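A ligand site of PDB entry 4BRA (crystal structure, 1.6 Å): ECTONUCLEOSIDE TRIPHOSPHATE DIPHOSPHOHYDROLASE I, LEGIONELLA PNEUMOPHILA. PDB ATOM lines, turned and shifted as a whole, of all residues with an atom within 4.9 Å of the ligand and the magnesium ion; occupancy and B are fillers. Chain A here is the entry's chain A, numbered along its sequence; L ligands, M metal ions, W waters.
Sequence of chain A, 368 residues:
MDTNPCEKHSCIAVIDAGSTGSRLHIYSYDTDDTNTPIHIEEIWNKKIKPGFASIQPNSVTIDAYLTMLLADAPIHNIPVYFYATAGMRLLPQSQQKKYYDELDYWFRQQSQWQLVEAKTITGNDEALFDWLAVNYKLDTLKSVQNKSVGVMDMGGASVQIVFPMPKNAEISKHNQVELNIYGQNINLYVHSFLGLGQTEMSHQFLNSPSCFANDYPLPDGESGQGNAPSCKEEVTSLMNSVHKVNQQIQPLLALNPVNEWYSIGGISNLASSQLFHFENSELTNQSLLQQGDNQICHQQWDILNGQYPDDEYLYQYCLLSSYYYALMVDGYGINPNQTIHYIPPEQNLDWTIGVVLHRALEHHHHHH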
ATOM      1  N   ASP A  16      -6.019   6.128 -12.314  1.00  0.00           N
ATOM      2  CA  ASP A  16      -5.747   4.755 -11.873  1.00  0.00           C
ATOM      3  C   ASP A  16      -4.265   4.716 -11.593  1.00  0.00           C
ATOM      4  O   ASP A  16      -3.474   4.664 -12.528  1.00  0.00           O
ATOM      5  CB  ASP A  16      -6.140   3.790 -13.018  1.00  0.00           C
ATOM      6  CG  ASP A  16      -5.622   2.403 -12.842  1.00  0.00           C
ATOM      7  OD1 ASP A  16      -5.082   2.058 -11.764  1.00  0.00           O
ATOM      8  OD2 ASP A  16      -5.769   1.602 -13.791  1.00  0.00           O
ATOM      9  N   GLY A  18      -1.925   2.435 -10.633  1.00  0.00           N
ATOM     10  CA  GLY A  18      -1.687   1.011 -10.538  1.00  0.00           C
ATOM     11  C   GLY A  18      -0.244   0.646 -10.243  1.00  0.00           C
ATOM     12  O   GLY A  18       0.654   1.505 -10.262  1.00  0.00           O
ATOM     13  N   SER A  19      -0.075  -0.647  -9.918  1.00  0.00           N
ATOM     14  CA  SER A  19       1.255  -1.102  -9.489  1.00  0.00           C
ATOM     15  C   SER A  19       2.310  -0.868 -10.584  1.00  0.00           C
ATOM     16  O   SER A  19       3.506  -0.669 -10.229  1.00  0.00           O
ATOM     17  CB  SER A  19       1.239  -2.582  -9.076  1.00  0.00           C
ATOM     18  OG  SER A  19       1.136  -3.455 -10.233  1.00  0.00           O
ATOM     19  N   THR A  20       1.906  -0.920 -11.893  1.00  0.00           N
ATOM     20  CA  THR A  20       2.849  -0.770 -12.997  1.00  0.00           C
ATOM     21  C   THR A  20       2.925   0.577 -13.689  1.00  0.00           C
ATOM     22  O   THR A  20       3.822   0.830 -14.565  1.00  0.00           O
ATOM     23  CB  THR A  20       2.776  -1.899 -14.047  1.00  0.00           C
ATOM     24  OG1 THR A  20       1.587  -1.763 -14.859  1.00  0.00           O
ATOM     25  CG2 THR A  20       2.861  -3.356 -13.388  1.00  0.00           C
ATOM     26  N   GLY A  21       1.992   1.453 -13.325  1.00  0.00           N
ATOM     27  CA  GLY A  21       2.000   2.708 -13.969  1.00  0.00           C
ATOM     28  C   GLY A  21       0.696   3.464 -13.603  1.00  0.00           C
ATOM     29  O   GLY A  21      -0.211   2.907 -12.923  1.00  0.00           O
ATOM     30  N   ARG A  23      -2.631   5.900 -14.919  1.00  0.00           N
ATOM     31  CA  ARG A  23      -3.358   6.287 -16.133  1.00  0.00           C
ATOM     32  C   ARG A  23      -4.379   7.359 -15.777  1.00  0.00           C
ATOM     33  O   ARG A  23      -5.238   7.168 -14.902  1.00  0.00           O
ATOM     34  CB  ARG A  23      -4.036   5.079 -16.840  1.00  0.00           C
ATOM     35  CG  ARG A  23      -3.108   3.911 -17.108  1.00  0.00           C
ATOM     36  CD  ARG A  23      -3.189   2.919 -15.954  1.00  0.00           C
ATOM     37  NE  ARG A  23      -2.016   2.067 -15.930  1.00  0.00           N
ATOM     38  CZ  ARG A  23      -1.867   1.021 -15.113  1.00  0.00           C
ATOM     39  NH1 ARG A  23      -2.864   0.671 -14.295  1.00  0.00           N
ATOM     40  NH2 ARG A  23      -0.737   0.283 -15.149  1.00  0.00           N
ATOM     41  N   THR A  85      -4.019   1.508  -6.264  1.00  0.00           N
ATOM     42  CA  THR A  85      -4.449   0.136  -6.032  1.00  0.00           C
ATOM     43  C   THR A  85      -3.335  -0.678  -5.377  1.00  0.00           C
ATOM     44  O   THR A  85      -2.670  -0.190  -4.452  1.00  0.00           O
ATOM     45  CB  THR A  85      -4.975  -0.512  -7.333  1.00  0.00           C
ATOM     46  OG1 THR A  85      -4.022  -0.378  -8.390  1.00  0.00           O
ATOM     47  CG2 THR A  85      -6.289   0.247  -7.741  1.00  0.00           C
ATOM     48  N   ALA A  86      -3.103  -1.881  -5.906  1.00  0.00           N
ATOM     49  CA  ALA A  86      -2.263  -2.839  -5.151  1.00  0.00           C
ATOM     50  C   ALA A  86      -0.793  -2.415  -4.947  1.00  0.00           C
ATOM     51  O   ALA A  86      -0.200  -2.879  -3.956  1.00  0.00           O
ATOM     52  CB  ALA A  86      -2.360  -4.242  -5.706  1.00  0.00           C
ATOM     53  N   GLY A  87      -0.212  -1.603  -5.849  1.00  0.00           N
ATOM     54  CA  GLY A  87       1.239  -1.218  -5.636  1.00  0.00           C
ATOM     55  C   GLY A  87       1.308  -0.468  -4.295  1.00  0.00           C
ATOM     56  O   GLY A  87       2.194  -0.713  -3.481  1.00  0.00           O
ATOM     57  N   GLU A 126     -11.909  -1.782  -5.454  1.00  0.00           N
ATOM     58  CA  GLU A 126     -11.367  -1.906  -6.830  1.00  0.00           C
ATOM     59  C   GLU A 126     -12.193  -2.935  -7.636  1.00  0.00           C
ATOM     60  O   GLU A 126     -12.536  -2.661  -8.832  1.00  0.00           O
ATOM     61  CB  GLU A 126      -9.881  -2.326  -6.739  1.00  0.00           C
ATOM     62  CG  GLU A 126      -9.115  -2.285  -8.024  1.00  0.00           C
ATOM     63  CD  GLU A 126      -7.688  -2.738  -7.766  1.00  0.00           C
ATOM     64  OE1 GLU A 126      -7.323  -2.945  -6.567  1.00  0.00           O
ATOM     65  OE2 GLU A 126      -6.919  -2.898  -8.755  1.00  0.00           O
ATOM     66  N   ASP A 153     -10.093  -8.876 -12.996  1.00  0.00           N
ATOM     67  CA  ASP A 153      -9.144  -7.797 -13.377  1.00  0.00           C
ATOM     68  C   ASP A 153      -7.824  -8.375 -13.014  1.00  0.00           C
ATOM     69  O   ASP A 153      -7.571  -8.665 -11.861  1.00  0.00           O
ATOM     70  CB  ASP A 153      -9.464  -6.503 -12.573  1.00  0.00           C
ATOM     71  CG  ASP A 153      -8.476  -5.336 -12.848  1.00  0.00           C
ATOM     72  OD1 ASP A 153      -7.423  -5.552 -13.535  1.00  0.00           O
ATOM     73  OD2 ASP A 153      -8.798  -4.178 -12.396  1.00  0.00           O
ATOM     74  N   MET A 154      -7.039  -8.615 -14.043  1.00  0.00           N
ATOM     75  CA  MET A 154      -5.767  -9.295 -13.925  1.00  0.00           C
ATOM     76  C   MET A 154      -4.606  -8.254 -13.854  1.00  0.00           C
ATOM     77  O   MET A 154      -3.990  -7.911 -14.881  1.00  0.00           O
ATOM     78  CB  MET A 154      -5.601 -10.171 -15.189  1.00  0.00           C
ATOM     79  CG  MET A 154      -6.633 -11.266 -15.344  1.00  0.00           C
ATOM     80  SD  MET A 154      -6.728 -12.349 -13.894  1.00  0.00           S
ATOM     81  CE  MET A 154      -7.861 -13.590 -14.653  1.00  0.00           C
ATOM     82  N   GLY A 155      -4.348  -7.734 -12.669  1.00  0.00           N
ATOM     83  CA  GLY A 155      -3.390  -6.646 -12.484  1.00  0.00           C
ATOM     84  C   GLY A 155      -1.967  -7.202 -12.216  1.00  0.00           C
ATOM     85  O   GLY A 155      -1.724  -8.393 -12.273  1.00  0.00           O
ATOM     86  N   GLY A 156      -1.089  -6.272 -11.921  1.00  0.00           N
ATOM     87  CA  GLY A 156       0.312  -6.566 -11.760  1.00  0.00           C
ATOM     88  C   GLY A 156       0.594  -6.918 -10.318  1.00  0.00           C
ATOM     89  O   GLY A 156       1.495  -7.756 -10.040  1.00  0.00           O
ATOM     90  N   ALA A 157      -0.180  -6.378  -9.363  1.00  0.00           N
ATOM     91  CA  ALA A 157       0.079  -6.763  -7.975  1.00  0.00           C
ATOM     92  C   ALA A 157      -1.046  -7.482  -7.256  1.00  0.00           C
ATOM     93  O   ALA A 157      -0.803  -8.258  -6.333  1.00  0.00           O
ATOM     94  CB  ALA A 157       0.581  -5.555  -7.166  1.00  0.00           C
ATOM     95  N   SER A 158      -2.337  -7.259  -7.691  1.00  0.00           N
ATOM     96  CA  SER A 158      -3.416  -8.037  -7.185  1.00  0.00           C
ATOM     97  C   SER A 158      -4.276  -8.407  -8.368  1.00  0.00           C
ATOM     98  O   SER A 158      -4.154  -7.835  -9.477  1.00  0.00           O
ATOM     99  CB  SER A 158      -4.290  -7.263  -6.122  1.00  0.00           C
ATOM    100  OG  SER A 158      -5.004  -6.195  -6.756  1.00  0.00           O
ATOM    101  N   GLN A 198       0.363 -10.333 -11.615  1.00  0.00           N
ATOM    102  CA  GLN A 198       1.364 -10.989 -12.453  1.00  0.00           C
ATOM    103  C   GLN A 198       2.818 -10.663 -12.034  1.00  0.00           C
ATOM    104  O   GLN A 198       3.663 -11.561 -12.036  1.00  0.00           O
ATOM    105  CB  GLN A 198       1.086 -10.840 -13.942  1.00  0.00           C
ATOM    106  CG  GLN A 198       1.289  -9.523 -14.519  1.00  0.00           C
ATOM    107  CD  GLN A 198       1.362  -9.599 -16.037  1.00  0.00           C
ATOM    108  OE1 GLN A 198       0.308  -9.747 -16.791  1.00  0.00           O
ATOM    109  NE2 GLN A 198       2.620  -9.540 -16.537  1.00  0.00           N
ATOM    110  N   THR A 199       3.064  -9.432 -11.559  1.00  0.00           N
ATOM    111  CA  THR A 199       4.461  -9.063 -11.291  1.00  0.00           C
ATOM    112  C   THR A 199       4.836  -9.763 -10.014  1.00  0.00           C
ATOM    113  O   THR A 199       5.944 -10.341  -9.944  1.00  0.00           O
ATOM    114  CB  THR A 199       4.603  -7.529 -11.071  1.00  0.00           C
ATOM    115  OG1 THR A 199       4.210  -6.843 -12.254  1.00  0.00           O
ATOM    116  CG2 THR A 199       6.065  -7.117 -10.723  1.00  0.00           C
ATOM    117  N   GLY A 265      -7.418  -5.701 -17.366  1.00  0.00           N
ATOM    118  CA  GLY A 265      -6.003  -5.827 -16.862  1.00  0.00           C
ATOM    119  C   GLY A 265      -5.069  -6.284 -17.951  1.00  0.00           C
ATOM    120  O   GLY A 265      -5.400  -6.379 -19.162  1.00  0.00           O
ATOM    121  N   GLY A 266      -3.884  -6.724 -17.509  1.00  0.00           N
ATOM    122  CA  GLY A 266      -2.795  -6.969 -18.475  1.00  0.00           C
ATOM    123  C   GLY A 266      -3.017  -8.210 -19.324  1.00  0.00           C
ATOM    124  O   GLY A 266      -2.352  -8.388 -20.327  1.00  0.00           O
ATOM    125  N   ASN A 269      -3.345  -7.408 -22.945  1.00  0.00           N
ATOM    126  CA  ASN A 269      -2.097  -7.189 -23.653  1.00  0.00           C
ATOM    127  C   ASN A 269      -1.463  -8.512 -24.095  1.00  0.00           C
ATOM    128  O   ASN A 269      -0.981  -8.624 -25.207  1.00  0.00           O
ATOM    129  CB  ASN A 269      -1.129  -6.359 -22.800  1.00  0.00           C
ATOM    130  CG  ASN A 269      -1.734  -5.036 -22.405  1.00  0.00           C
ATOM    131  OD1 ASN A 269      -2.281  -4.893 -21.323  1.00  0.00           O
ATOM    132  ND2 ASN A 269      -1.748  -4.096 -23.339  1.00  0.00           N
ATOM    133  N   LEU A 270      -1.495  -9.517 -23.233  1.00  0.00           N
ATOM    134  CA  LEU A 270      -0.968 -10.829 -23.573  1.00  0.00           C
ATOM    135  C   LEU A 270      -1.774 -11.449 -24.724  1.00  0.00           C
ATOM    136  O   LEU A 270      -1.193 -11.882 -25.728  1.00  0.00           O
ATOM    137  CB  LEU A 270      -1.046 -11.736 -22.338  1.00  0.00           C
ATOM    138  CG  LEU A 270      -0.614 -13.221 -22.533  1.00  0.00           C
ATOM    139  CD1 LEU A 270       0.885 -13.324 -22.630  1.00  0.00           C
ATOM    140  CD2 LEU A 270      -1.088 -14.122 -21.378  1.00  0.00           C
ATOM    141  N   TYR A 313       8.176  -7.924 -22.872  1.00  0.00           N
ATOM    142  CA  TYR A 313       7.275  -8.801 -22.102  1.00  0.00           C
ATOM    143  C   TYR A 313       7.327 -10.259 -22.556  1.00  0.00           C
ATOM    144  O   TYR A 313       6.952 -11.182 -21.773  1.00  0.00           O
ATOM    145  CB  TYR A 313       5.839  -8.283 -22.215  1.00  0.00           C
ATOM    146  CG  TYR A 313       5.718  -6.822 -21.745  1.00  0.00           C
ATOM    147  CD1 TYR A 313       5.717  -6.530 -20.390  1.00  0.00           C
ATOM    148  CD2 TYR A 313       5.707  -5.764 -22.649  1.00  0.00           C
ATOM    149  CE1 TYR A 313       5.631  -5.233 -19.911  1.00  0.00           C
ATOM    150  CE2 TYR A 313       5.608  -4.419 -22.211  1.00  0.00           C
ATOM    151  CZ  TYR A 313       5.559  -4.165 -20.836  1.00  0.00           C
ATOM    152  OH  TYR A 313       5.489  -2.874 -20.324  1.00  0.00           O
ATOM    153  N   GLN A 316       8.270 -13.658 -20.680  1.00  0.00           N
ATOM    154  CA  GLN A 316       7.434 -14.069 -19.611  1.00  0.00           C
ATOM    155  C   GLN A 316       6.186 -14.771 -20.136  1.00  0.00           C
ATOM    156  O   GLN A 316       5.357 -15.193 -19.330  1.00  0.00           O
ATOM    157  CB  GLN A 316       6.956 -12.836 -18.835  1.00  0.00           C
ATOM    158  CG  GLN A 316       6.803 -13.140 -17.402  1.00  0.00           C
ATOM    159  CD  GLN A 316       6.464 -11.891 -16.503  1.00  0.00           C
ATOM    160  OE1 GLN A 316       6.667 -11.938 -15.318  1.00  0.00           O
ATOM    161  NE2 GLN A 316       5.979 -10.785 -17.115  1.00  0.00           N
ATOM    162  N   TYR A 317       6.014 -14.876 -21.462  1.00  0.00           N
ATOM    163  CA  TYR A 317       4.699 -15.377 -21.954  1.00  0.00           C
ATOM    164  C   TYR A 317       4.421 -16.869 -21.648  1.00  0.00           C
ATOM    165  O   TYR A 317       3.252 -17.276 -21.553  1.00  0.00           O
ATOM    166  CB  TYR A 317       4.595 -15.137 -23.469  1.00  0.00           C
ATOM    167  CG  TYR A 317       4.236 -13.712 -23.853  1.00  0.00           C
ATOM    168  CD1 TYR A 317       4.162 -12.684 -22.892  1.00  0.00           C
ATOM    169  CD2 TYR A 317       4.073 -13.364 -25.195  1.00  0.00           C
ATOM    170  CE1 TYR A 317       3.837 -11.391 -23.248  1.00  0.00           C
ATOM    171  CE2 TYR A 317       3.783 -12.067 -25.562  1.00  0.00           C
ATOM    172  CZ  TYR A 317       3.659 -11.089 -24.575  1.00  0.00           C
ATOM    173  OH  TYR A 317       3.371  -9.807 -24.981  1.00  0.00           O
ATOM    174  N   LEU A 320       3.238 -16.532 -18.034  1.00  0.00           N
ATOM    175  CA  LEU A 320       1.933 -15.857 -17.880  1.00  0.00           C
ATOM    176  C   LEU A 320       0.781 -16.717 -18.396  1.00  0.00           C
ATOM    177  O   LEU A 320      -0.306 -16.765 -17.791  1.00  0.00           O
ATOM    178  CB  LEU A 320       1.883 -14.514 -18.601  1.00  0.00           C
ATOM    179  CG  LEU A 320       2.888 -13.501 -17.994  1.00  0.00           C
ATOM    180  CD1 LEU A 320       2.703 -12.173 -18.673  1.00  0.00           C
ATOM    181  CD2 LEU A 320       2.632 -13.256 -16.515  1.00  0.00           C
ATOM    182  N   TRP A 351     -10.945   0.174 -14.367  1.00  0.00           N
ATOM    183  CA  TRP A 351     -12.061   0.283 -13.409  1.00  0.00           C
ATOM    184  C   TRP A 351     -12.482   1.737 -13.207  1.00  0.00           C
ATOM    185  O   TRP A 351     -13.426   2.009 -12.486  1.00  0.00           O
ATOM    186  CB  TRP A 351     -11.663  -0.370 -12.097  1.00  0.00           C
ATOM    187  CG  TRP A 351     -10.308   0.071 -11.644  1.00  0.00           C
ATOM    188  CD1 TRP A 351      -9.113  -0.663 -11.759  1.00  0.00           C
ATOM    189  CD2 TRP A 351      -9.954   1.321 -10.989  1.00  0.00           C
ATOM    190  NE1 TRP A 351      -8.066   0.088 -11.215  1.00  0.00           N
ATOM    191  CE2 TRP A 351      -8.528   1.287 -10.760  1.00  0.00           C
ATOM    192  CE3 TRP A 351     -10.682   2.447 -10.544  1.00  0.00           C
ATOM    193  CZ2 TRP A 351      -7.852   2.361 -10.121  1.00  0.00           C
ATOM    194  CZ3 TRP A 351      -9.982   3.510  -9.962  1.00  0.00           C
ATOM    195  CH2 TRP A 351      -8.620   3.444  -9.745  1.00  0.00           C
HETATM  196  P1  LIG L   1      -2.606  -3.312 -10.154  1.00  0.00           P
HETATM  197  O1  LIG L   1      -2.323  -2.097  -9.266  1.00  0.00           O
HETATM  198  O2  LIG L   1      -4.035  -3.304 -10.751  1.00  0.00           O
HETATM  199  O3  LIG L   1      -2.358  -4.578  -9.406  1.00  0.00           O
HETATM  200  P2  LIG L   1      -1.676  -2.577 -12.892  1.00  0.00           P
HETATM  201  O4  LIG L   1      -3.028  -1.862 -13.072  1.00  0.00           O
HETATM  202  O5  LIG L   1      -0.486  -1.646 -13.172  1.00  0.00           O
HETATM  203  N1  LIG L   1      -1.435  -3.391 -11.432  1.00  0.00           N
HETATM  204  P3  LIG L   1      -2.163  -3.830 -15.423  1.00  0.00           P
HETATM  205  O6  LIG L   1      -1.888  -2.546 -16.131  1.00  0.00           O
HETATM  206  O7  LIG L   1      -3.502  -4.434 -15.417  1.00  0.00           O
HETATM  207  O8  LIG L   1      -1.606  -3.827 -13.954  1.00  0.00           O
HETATM  208  O9  LIG L   1      -1.206  -4.984 -16.040  1.00  0.00           O
HETATM  209  C1  LIG L   1       0.181  -4.728 -16.091  1.00  0.00           C
HETATM  210  C2  LIG L   1       0.913  -5.878 -16.759  1.00  0.00           C
HETATM  211  O10 LIG L   1       0.419  -5.992 -18.090  1.00  0.00           O
HETATM  212  C3  LIG L   1       2.314  -5.456 -17.069  1.00  0.00           C
HETATM  213  O11 LIG L   1       3.200  -5.819 -16.023  1.00  0.00           O
HETATM  214  C4  LIG L   1       2.723  -6.281 -18.251  1.00  0.00           C
HETATM  215  O12 LIG L   1       3.137  -7.601 -17.867  1.00  0.00           O
HETATM  216  C5  LIG L   1       1.466  -6.420 -19.014  1.00  0.00           C
HETATM  217  N2  LIG L   1       1.673  -5.515 -20.156  1.00  0.00           N
HETATM  218  C6  LIG L   1       1.627  -4.149 -20.177  1.00  0.00           C
HETATM  219  N3  LIG L   1       1.872  -3.666 -21.464  1.00  0.00           N
HETATM  220  C7  LIG L   1       2.081  -4.738 -22.241  1.00  0.00           C
HETATM  221  C8  LIG L   1       2.404  -4.942 -23.662  1.00  0.00           C
HETATM  222  N4  LIG L   1       2.539  -3.830 -24.459  1.00  0.00           N
HETATM  223  N5  LIG L   1       2.575  -6.249 -24.088  1.00  0.00           N
HETATM  224  C9  LIG L   1       2.443  -7.320 -23.262  1.00  0.00           C
HETATM  225  N6  LIG L   1       2.169  -7.183 -21.954  1.00  0.00           N
HETATM  226  C10 LIG L   1       1.999  -5.946 -21.390  1.00  0.00           C
HETATM  227 MG    MG M   1      -4.865  -2.229 -12.255  1.00  0.00          MG
HETATM  228  O   HOH W   1      -5.594  -5.492 -10.254  1.00  0.00           O
HETATM  229  O   HOH W   2       2.199  -2.011 -17.602  1.00  0.00           O
HETATM  230  O   HOH W   3       5.598  -4.642 -15.941  1.00  0.00           O
HETATM  231  O   HOH W   4      -4.626  -1.458 -16.242  1.00  0.00           O
HETATM  232  O   HOH W   5      -4.930  -0.420 -11.057  1.00  0.00           O
HETATM  233  O   HOH W   6      -0.966  -1.961 -18.425  1.00  0.00           O
HETATM  234  O   HOH W   7      -5.788  -1.028 -13.773  1.00  0.00           O
HETATM  235  O   HOH W   8      -6.752  -2.675 -11.446  1.00  0.00           O
HETATM  236  O   HOH W   9      -4.605  -3.719  -7.721  1.00  0.00           O
HETATM  237  O   HOH W  10      -1.323  -7.816 -15.534  1.00  0.00           O
HETATM  238  O   HOH W  11      -5.212  -3.939 -13.463  1.00  0.00           O
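No residue comes within 4 Å of the magnesium ion.
Water W7 bridges the side-chain carboxylate (OD2) of Asp 16 (2.6 Å) and the guanidinium group (NH1) of Arg 23 (3.4 Å).
Water W8 lies within hydrogen-bond range of the side-chain carboxylate of Glu 126 (2.7 Å), the side-chain carboxylate of Asp 153 (2.7 Å) and the indole nitrogen of Trp 351 (3.1 Å).
Water W11 bridges an oxygen (O7) of the ligand and the side-chain carboxylate of Asp 153.
Water W1 lies within hydrogen-bond range of O of Ser 158 (2.9 Å), OE2 of Glu 126 (3.3 Å) and O3 of the ligand (3.5 Å).
Water W9 lies within hydrogen-bond range of OE2 of Glu 126 (2.7 Å), OG of Ser 158 (2.7 Å), O3 of the ligand (2.9 Å), N of Ala 86 (3.0 Å) and OG1 of Thr 85 (3.5 Å).
Water W4 bridges O6 of the ligand (2.9 Å) and NH1 of Arg 23 (3.4 Å).
O12 of the ligand lies within hydrogen-bond range of NE2 of Gln 198, 2.4 Å away.
O1 of the ligand sits at hydrogen-bond distance from OG1 of Thr 85, 2.6 Å away.
O5 of the ligand sits at hydrogen-bond distance from N of Thr 20 (2.8 Å).
OG1 of Thr 20 lies within hydrogen-bond range of O5 of the ligand (2.7 Å).
The backbone NH of Ser 19 lies within hydrogen-bond range of an oxygen (O1) of the ligand, 2.8 Å away.
N1 of the ligand sits at hydrogen-bond distance from OG of Ser 19, at 2.8 Å.
The guanidinium group of Arg 23 is in salt-bridge range of an oxygen (O5) of the ligand (2.8 Å).
O3 of the ligand lies within hydrogen-bond range of N of Ala 157 (2.8 Å).
The backbone NH of Gly 156 sits at hydrogen-bond distance from an oxygen (O8) of the ligand (3.2 Å).
N of Gly 266 lies within hydrogen-bond range of O7 of the ligand.
O3 of the ligand sits at hydrogen-bond distance from N of Ser 158, at 3.2 Å.
An oxygen (O1) of the ligand is in hydrogen-bond range of the backbone NH (N) of Ala 86 (3.5 Å).
The backbone NH (N) of Gln 198 lies within hydrogen-bond range of the backbone carbonyl oxygen (O) of Gly 156 (3.2 Å).
N of Gln 198 is in hydrogen-bond range of O of Gly 155 (2.9 Å).
OG1 of Thr 20 sits at hydrogen-bond distance from NH2 of Arg 23, 3.1 Å away.
The side-chain hydroxyl (OG) of Ser 19 is in hydrogen-bond range of the backbone NH (N) of Ala 157, 3.3 Å away.
O of Gly 21 sits close to NH2 of Arg 23 (3.5 Å).
The guanidinium group of Arg 23 is in salt-bridge range of the side-chain carboxylate of Asp 16.
N of Gly 266 is in hydrogen-bond range of O of Met 154 (2.9 Å).
The backbone NH (N) of Gly 18 sits at hydrogen-bond distance from the side-chain carboxylate (OD1) of Asp 16, at 3.4 Å.
Residues that only touch the ligand: Tyr 317 (3.2 Å), Gly 265 (3.2 Å), Gly 18 (3.4 Å), Asn 269 (3.5 Å), Tyr 313 (3.5 Å), Glu 126 (3.5 Å), Met 154 (3.6 Å), Gly 155 (3.6 Å) and Gly 21 (3.97 Å).
Hydrophobic or aromatic side chains within 4 Å of the ligand: Ala 86, Ala 157 and Tyr 313.
19 residues have an atom within 4 Å of the ligand: Gly 18, Ser 19, Thr 20, Gly 21, Arg 23, Thr 85, Ala 86, Glu 126, Met 154, Gly 155, Gly 156, Ala 157, Ser 158, Gln 198, Gly 265, Gly 266, Asn 269, Tyr 313 and Tyr 317.
The nearest printed residue that does not touch the ligand is Thr 199 (4.03 Å).
The magnesium ion is bound by O2 of the ligand, O4 of the ligand, water W8, water W11, water W7 and water W5.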
